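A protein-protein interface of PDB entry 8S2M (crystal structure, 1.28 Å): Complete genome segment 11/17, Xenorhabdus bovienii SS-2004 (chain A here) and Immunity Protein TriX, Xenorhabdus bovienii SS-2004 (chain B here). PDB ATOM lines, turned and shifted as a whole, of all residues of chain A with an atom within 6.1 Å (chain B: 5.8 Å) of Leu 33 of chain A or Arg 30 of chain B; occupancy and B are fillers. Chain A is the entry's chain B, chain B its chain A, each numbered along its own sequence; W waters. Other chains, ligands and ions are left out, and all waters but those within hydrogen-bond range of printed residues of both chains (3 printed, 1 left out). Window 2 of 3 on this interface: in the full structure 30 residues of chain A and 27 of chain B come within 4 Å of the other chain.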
ATOM      1  N   ARG A  16      18.286 -12.685 -11.661  1.00  0.00           N
ATOM      2  CA  ARG A  16      18.744 -13.186 -10.371  1.00  0.00           C
ATOM      3  C   ARG A  16      18.606 -14.699 -10.334  1.00  0.00           C
ATOM      4  O   ARG A  16      17.538 -15.233 -10.669  1.00  0.00           O
ATOM      5  CB  ARG A  16      17.879 -12.592  -9.257  1.00  0.00           C
ATOM      6  CG  ARG A  16      18.115 -13.200  -7.908  1.00  0.00           C
ATOM      7  CD  ARG A  16      17.232 -12.541  -6.866  1.00  0.00           C
ATOM      8  NE  ARG A  16      17.329 -13.269  -5.615  1.00  0.00           N
ATOM      9  CZ  ARG A  16      18.319 -13.109  -4.750  1.00  0.00           C
ATOM     10  NH1 ARG A  16      19.255 -12.188  -4.937  1.00  0.00           N
ATOM     11  NH2 ARG A  16      18.366 -13.874  -3.662  1.00  0.00           N
ATOM     12  N   ARG A  20      14.467 -20.578  -4.751  1.00  0.00           N
ATOM     13  CA  ARG A  20      13.122 -20.584  -4.204  1.00  0.00           C
ATOM     14  C   ARG A  20      12.084 -20.719  -5.311  1.00  0.00           C
ATOM     15  O   ARG A  20      12.295 -20.289  -6.449  1.00  0.00           O
ATOM     16  CB  ARG A  20      12.875 -19.318  -3.386  1.00  0.00           C
ATOM     17  CG  ARG A  20      13.572 -19.365  -2.057  1.00  0.00           C
ATOM     18  CD  ARG A  20      13.509 -18.051  -1.315  1.00  0.00           C
ATOM     19  NE  ARG A  20      14.208 -16.981  -2.015  1.00  0.00           N
ATOM     20  CZ  ARG A  20      14.214 -15.720  -1.611  1.00  0.00           C
ATOM     21  NH1 ARG A  20      13.563 -15.342  -0.521  1.00  0.00           N
ATOM     22  NH2 ARG A  20      14.897 -14.820  -2.313  1.00  0.00           N
ATOM     23  N   GLU A  31      12.813 -10.213  -0.758  1.00  0.00           N
ATOM     24  CA  GLU A  31      13.005  -9.417   0.446  1.00  0.00           C
ATOM     25  C   GLU A  31      14.463  -9.470   0.897  1.00  0.00           C
ATOM     26  O   GLU A  31      15.190 -10.413   0.589  1.00  0.00           O
ATOM     27  CB  GLU A  31      12.083  -9.932   1.552  1.00  0.00           C
ATOM     28  CG  GLU A  31      10.618  -9.943   1.107  1.00  0.00           C
ATOM     29  CD  GLU A  31       9.647 -10.274   2.223  1.00  0.00           C
ATOM     30  OE1 GLU A  31       9.331  -9.376   3.033  1.00  0.00           O
ATOM     31  OE2 GLU A  31       9.176 -11.432   2.273  1.00  0.00           O
ATOM     32  N   THR A  32      14.892  -8.433   1.609  1.00  0.00           N
ATOM     33  CA  THR A  32      16.257  -8.359   2.114  1.00  0.00           C
ATOM     34  C   THR A  32      16.341  -8.957   3.517  1.00  0.00           C
ATOM     35  O   THR A  32      15.333  -9.176   4.187  1.00  0.00           O
ATOM     36  CB  THR A  32      16.765  -6.917   2.122  1.00  0.00           C
ATOM     37  OG1 THR A  32      16.060  -6.179   3.118  1.00  0.00           O
ATOM     38  CG2 THR A  32      16.537  -6.250   0.770  1.00  0.00           C
ATOM     39  N   LEU A  33      17.577  -9.202   3.969  1.00  0.00           N
ATOM     40  CA  LEU A  33      17.815  -9.868   5.244  1.00  0.00           C
ATOM     41  C   LEU A  33      18.157  -8.909   6.377  1.00  0.00           C
ATOM     42  O   LEU A  33      18.205  -9.336   7.535  1.00  0.00           O
ATOM     43  CB  LEU A  33      18.939 -10.905   5.095  1.00  0.00           C
ATOM     44  CG  LEU A  33      18.610 -12.123   4.221  1.00  0.00           C
ATOM     45  CD1 LEU A  33      19.854 -12.992   4.017  1.00  0.00           C
ATOM     46  CD2 LEU A  33      17.476 -12.938   4.824  1.00  0.00           C
ATOM     47  N   GLY A  34      18.422  -7.641   6.081  1.00  0.00           N
ATOM     48  CA  GLY A  34      18.732  -6.691   7.123  1.00  0.00           C
ATOM     49  C   GLY A  34      18.585  -5.260   6.657  1.00  0.00           C
ATOM     50  O   GLY A  34      18.364  -4.986   5.477  1.00  0.00           O
ATOM     51  N   PRO A  35      18.729  -4.314   7.582  1.00  0.00           N
ATOM     52  CA  PRO A  35      18.475  -2.901   7.275  1.00  0.00           C
ATOM     53  C   PRO A  35      19.671  -2.055   6.848  1.00  0.00           C
ATOM     54  O   PRO A  35      19.471  -0.865   6.581  1.00  0.00           O
ATOM     55  CB  PRO A  35      17.912  -2.403   8.613  1.00  0.00           C
ATOM     56  CG  PRO A  35      18.745  -3.140   9.624  1.00  0.00           C
ATOM     57  CD  PRO A  35      18.937  -4.531   9.025  1.00  0.00           C
ATOM     58  N   PRO A  50      23.935  -7.586   7.929  1.00  0.00           N
ATOM     59  CA  PRO A  50      23.041  -7.959   6.822  1.00  0.00           C
ATOM     60  C   PRO A  50      22.519  -6.730   6.086  1.00  0.00           C
ATOM     61  O   PRO A  50      21.992  -5.793   6.690  1.00  0.00           O
ATOM     62  CB  PRO A  50      21.922  -8.749   7.512  1.00  0.00           C
ATOM     63  CG  PRO A  50      22.555  -9.262   8.764  1.00  0.00           C
ATOM     64  CD  PRO A  50      23.489  -8.165   9.210  1.00  0.00           C
ATOM     65  N   SER A  51      22.681  -6.733   4.767  1.00  0.00           N
ATOM     66  CA  SER A  51      22.457  -5.523   3.985  1.00  0.00           C
ATOM     67  C   SER A  51      21.038  -5.458   3.423  1.00  0.00           C
ATOM     68  O   SER A  51      20.389  -6.479   3.179  1.00  0.00           O
ATOM     69  CB  SER A  51      23.492  -5.422   2.863  1.00  0.00           C
ATOM     70  OG  SER A  51      23.154  -6.240   1.763  1.00  0.00           O
ATOM     71  N   ASP A  52      20.567  -4.235   3.213  1.00  0.00           N
ATOM     72  CA  ASP A  52      19.220  -3.971   2.699  1.00  0.00           C
ATOM     73  C   ASP A  52      19.211  -3.887   1.177  1.00  0.00           C
ATOM     74  O   ASP A  52      18.691  -2.943   0.593  1.00  0.00           O
ATOM     75  CB  ASP A  52      18.671  -2.689   3.322  1.00  0.00           C
ATOM     76  CG  ASP A  52      17.158  -2.578   3.220  1.00  0.00           C
ATOM     77  OD1 ASP A  52      16.478  -3.543   2.827  1.00  0.00           O
ATOM     78  OD2 ASP A  52      16.636  -1.501   3.563  1.00  0.00           O
ATOM     79  N   PHE A  53      19.810  -4.877   0.522  1.00  0.00           N
ATOM     80  CA  PHE A  53      19.843  -4.937  -0.933  1.00  0.00           C
ATOM     81  C   PHE A  53      19.585  -6.366  -1.375  1.00  0.00           C
ATOM     82  O   PHE A  53      20.051  -7.320  -0.738  1.00  0.00           O
ATOM     83  CB  PHE A  53      21.212  -4.538  -1.504  1.00  0.00           C
ATOM     84  CG  PHE A  53      21.667  -3.172  -1.107  1.00  0.00           C
ATOM     85  CD1 PHE A  53      21.324  -2.054  -1.855  1.00  0.00           C
ATOM     86  CD2 PHE A  53      22.454  -3.002   0.021  1.00  0.00           C
ATOM     87  CE1 PHE A  53      21.753  -0.796  -1.472  1.00  0.00           C
ATOM     88  CE2 PHE A  53      22.888  -1.754   0.403  1.00  0.00           C
ATOM     89  CZ  PHE A  53      22.538  -0.645  -0.345  1.00  0.00           C
ATOM     90  N   SER B  27      15.326 -24.445   4.952  1.00  0.00           N
ATOM     91  CA  SER B  27      13.938 -24.345   5.368  1.00  0.00           C
ATOM     92  C   SER B  27      13.356 -22.997   4.957  1.00  0.00           C
ATOM     93  O   SER B  27      14.082 -22.100   4.515  1.00  0.00           O
ATOM     94  CB  SER B  27      13.852 -24.518   6.891  1.00  0.00           C
ATOM     95  OG  SER B  27      14.336 -25.787   7.285  1.00  0.00           O
ATOM     96  N   PRO B  28      12.036 -22.820   5.079  1.00  0.00           N
ATOM     97  CA  PRO B  28      11.430 -21.534   4.717  1.00  0.00           C
ATOM     98  C   PRO B  28      12.023 -20.374   5.506  1.00  0.00           C
ATOM     99  O   PRO B  28      12.637 -20.547   6.561  1.00  0.00           O
ATOM    100  CB  PRO B  28       9.951 -21.739   5.070  1.00  0.00           C
ATOM    101  CG  PRO B  28       9.751 -23.191   4.838  1.00  0.00           C
ATOM    102  CD  PRO B  28      10.998 -23.827   5.380  1.00  0.00           C
ATOM    103  N   ASN B  29      11.832 -19.170   4.960  1.00  0.00           N
ATOM    104  CA  ASN B  29      12.246 -17.923   5.607  1.00  0.00           C
ATOM    105  C   ASN B  29      13.766 -17.811   5.724  1.00  0.00           C
ATOM    106  O   ASN B  29      14.282 -17.303   6.719  1.00  0.00           O
ATOM    107  CB  ASN B  29      11.569 -17.709   6.966  1.00  0.00           C
ATOM    108  CG  ASN B  29      10.059 -17.712   6.871  1.00  0.00           C
ATOM    109  OD1 ASN B  29       9.386 -18.536   7.492  1.00  0.00           O
ATOM    110  ND2 ASN B  29       9.515 -16.785   6.093  1.00  0.00           N
ATOM    111  N   ARG B  30      14.484 -18.295   4.707  1.00  0.00           N
ATOM    112  CA  ARG B  30      15.932 -18.119   4.578  1.00  0.00           C
ATOM    113  C   ARG B  30      16.730 -18.856   5.649  1.00  0.00           C
ATOM    114  O   ARG B  30      17.866 -18.478   5.940  1.00  0.00           O
ATOM    115  CB  ARG B  30      16.324 -16.635   4.558  1.00  0.00           C
ATOM    116  CG  ARG B  30      15.489 -15.783   3.630  1.00  0.00           C
ATOM    117  CD  ARG B  30      15.756 -16.115   2.181  1.00  0.00           C
ATOM    118  NE  ARG B  30      17.083 -15.683   1.757  1.00  0.00           N
ATOM    119  CZ  ARG B  30      17.344 -14.503   1.208  1.00  0.00           C
ATOM    120  NH1 ARG B  30      16.411 -13.571   1.099  1.00  0.00           N
ATOM    121  NH2 ARG B  30      18.572 -14.251   0.765  1.00  0.00           N
ATOM    122  N   HIS B  31      16.175 -19.906   6.240  1.00  0.00           N
ATOM    123  CA  HIS B  31      16.826 -20.609   7.340  1.00  0.00           C
ATOM    124  C   HIS B  31      17.719 -21.703   6.763  1.00  0.00           C
ATOM    125  O   HIS B  31      17.230 -22.676   6.175  1.00  0.00           O
ATOM    126  CB  HIS B  31      15.773 -21.184   8.288  1.00  0.00           C
ATOM    127  CG  HIS B  31      16.333 -22.040   9.389  1.00  0.00           C
ATOM    128  ND1 HIS B  31      15.531 -22.667  10.317  1.00  0.00           N
ATOM    129  CD2 HIS B  31      17.609 -22.365   9.715  1.00  0.00           C
ATOM    130  CE1 HIS B  31      16.287 -23.349  11.162  1.00  0.00           C
ATOM    131  NE2 HIS B  31      17.551 -23.181  10.818  1.00  0.00           N
ATOM    132  N   CYS B  32      19.028 -21.555   6.958  1.00  0.00           N
ATOM    133  CA  CYS B  32      20.010 -22.545   6.547  1.00  0.00           C
ATOM    134  C   CYS B  32      20.560 -23.226   7.794  1.00  0.00           C
ATOM    135  O   CYS B  32      21.046 -22.556   8.719  1.00  0.00           O
ATOM    136  CB  CYS B  32      21.155 -21.864   5.802  1.00  0.00           C
ATOM    137  SG  CYS B  32      20.658 -21.185   4.190  1.00  0.00           S
ATOM    138  N   ASP B  48      21.856 -20.252  10.298  1.00  0.00           N
ATOM    139  CA  ASP B  48      22.144 -18.915   9.804  1.00  0.00           C
ATOM    140  C   ASP B  48      21.302 -18.710   8.547  1.00  0.00           C
ATOM    141  O   ASP B  48      20.361 -19.470   8.296  1.00  0.00           O
ATOM    142  CB  ASP B  48      23.662 -18.750   9.591  1.00  0.00           C
ATOM    143  CG  ASP B  48      24.133 -17.324   9.775  1.00  0.00           C
ATOM    144  OD1 ASP B  48      23.635 -16.431   9.069  1.00  0.00           O
ATOM    145  OD2 ASP B  48      25.046 -17.102  10.598  1.00  0.00           O
ATOM    146  N   THR B  49      21.629 -17.691   7.759  1.00  0.00           N
ATOM    147  CA  THR B  49      20.888 -17.395   6.538  1.00  0.00           C
ATOM    148  C   THR B  49      21.671 -17.705   5.265  1.00  0.00           C
ATOM    149  O   THR B  49      21.166 -17.461   4.165  1.00  0.00           O
ATOM    150  CB  THR B  49      20.428 -15.933   6.530  1.00  0.00           C
ATOM    151  OG1 THR B  49      21.554 -15.089   6.776  1.00  0.00           O
ATOM    152  CG2 THR B  49      19.386 -15.700   7.624  1.00  0.00           C
ATOM    153  N   ASP B  50      22.893 -18.220   5.388  1.00  0.00           N
ATOM    154  CA  ASP B  50      23.659 -18.722   4.253  1.00  0.00           C
ATOM    155  C   ASP B  50      24.685 -19.713   4.779  1.00  0.00           C
ATOM    156  O   ASP B  50      25.050 -19.685   5.955  1.00  0.00           O
ATOM    157  CB  ASP B  50      24.302 -17.586   3.441  1.00  0.00           C
ATOM    158  CG  ASP B  50      25.554 -17.040   4.092  1.00  0.00           C
ATOM    159  OD1 ASP B  50      26.634 -17.649   3.957  1.00  0.00           O
ATOM    160  OD2 ASP B  50      25.453 -15.985   4.759  1.00  0.00           O
ATOM    161  N   ASP B  84      24.169 -14.151  -1.781  1.00  0.00           N
ATOM    162  CA  ASP B  84      22.732 -13.931  -1.874  1.00  0.00           C
ATOM    163  C   ASP B  84      22.072 -14.946  -2.802  1.00  0.00           C
ATOM    164  O   ASP B  84      21.102 -15.613  -2.417  1.00  0.00           O
ATOM    165  CB  ASP B  84      22.519 -12.496  -2.358  1.00  0.00           C
ATOM    166  CG  ASP B  84      21.099 -12.023  -2.242  1.00  0.00           C
ATOM    167  OD1 ASP B  84      20.257 -12.741  -1.667  1.00  0.00           O
ATOM    168  OD2 ASP B  84      20.816 -10.918  -2.735  1.00  0.00           O
ATOM    169  N   ASP B  87      22.868 -18.928  -1.611  1.00  0.00           N
ATOM    170  CA  ASP B  87      22.830 -19.248  -0.177  1.00  0.00           C
ATOM    171  C   ASP B  87      24.231 -19.531   0.361  1.00  0.00           C
ATOM    172  O   ASP B  87      24.434 -20.433   1.186  1.00  0.00           O
ATOM    173  CB  ASP B  87      21.871 -20.399   0.162  1.00  0.00           C
ATOM    174  CG  ASP B  87      20.429 -19.953   0.249  1.00  0.00           C
ATOM    175  OD1 ASP B  87      19.533 -20.789   0.010  1.00  0.00           O
ATOM    176  OD2 ASP B  87      20.193 -18.755   0.509  1.00  0.00           O
HETATM  177  O   HOH W   1      15.412 -12.042  -1.729  1.00  0.00           O
HETATM  178  O   HOH W   2      22.530  -8.919  -1.244  1.00  0.00           O
HETATM  179  O   HOH W   3      18.070 -11.630  -0.818  1.00  0.00           O
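Of the printed residues of chain B, Arg 20 of chain A touches Arg 30.
Leu 33 of chain A touches two residues of chain B.
Arg 30 of chain B touches just these residues of chain A: Arg 20 (3.6 Å), Glu 31 (3.4 Å) and Leu 33 (3.7 Å).
Of the printed residues of chain A, Thr 49 of chain B touches Leu 33 (3.9 Å).
Printed residues of chain A within 4 Å of Asp 84 of chain B: Arg 16.
The nearest printed residue of chain B that does not touch Leu 33 of chain A is Asp 84 of chain B (5.7 Å).
The nearest residue of chain A that does not touch Arg 30 of chain B is Arg 16 of chain A (4.4 Å).
The nearest printed residue of chain A that does not touch Asp 84 of chain B is Phe 53 of chain A (4.2 Å).
The side-chain carboxylate (OD1) of Asp 84 of chain B lies within salt-bridge range of the guanidinium group (NH2) of Arg 30 of chain B, 3.3 Å away.
The side-chain sulfur of Cys 32 of chain B is in hydrogen-bond range of the backbone carbonyl oxygen of Thr 49 of chain B (3.8 Å).
The side-chain carboxylate of Asp 48 of chain B lies within hydrogen-bond range of the side-chain hydroxyl of Thr 49 of chain B, at 3.4 Å.
Water W3 lies within hydrogen-bond range of OD1 of Asp 84 of chain B, NH2 of Arg 30 of chain B and O of Glu 31 of chain A.
Water W1 lies within hydrogen-bond range of O of Glu 31 of chain A (2.8 Å), NH2 of Arg 20 of chain A (2.9 Å) and NH1 of Arg 30 of chain B (3.4 Å).
Water W2 bridges O of Phe 53 of chain A and OD2 of Asp 84 of chain B.
Of the 11 printed residues of chain B, 3 touch a printed residue of chain A.
Printed residues of chain B that touch a printed residue of chain A: Arg 30, Thr 49 and Asp 84.
Of the 11 printed residues of chain A, 4 touch a printed residue of chain B.
Hydrophobic or aromatic side chains of chain A that line the printed part of chain B: Leu 33.
The guanidinium group (NH1) of Arg 30 of chain B sits at hydrogen-bond distance from the backbone carbonyl oxygen (O) of Glu 31 of chain A, at 3.4 Å.
The guanidinium group (NH2) of Arg 16 of chain A lies within salt-bridge range of the side-chain carboxylate (OD1) of Asp 84 of chain B (3.0 Å).
Among the printed residues, pairs that only touch across the chains: Arg 20 of chain A with Arg 30 of chain B, Leu 33 of chain A with Arg 30 of chain B and Leu 33 of chain A with Thr 49 of chain B.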
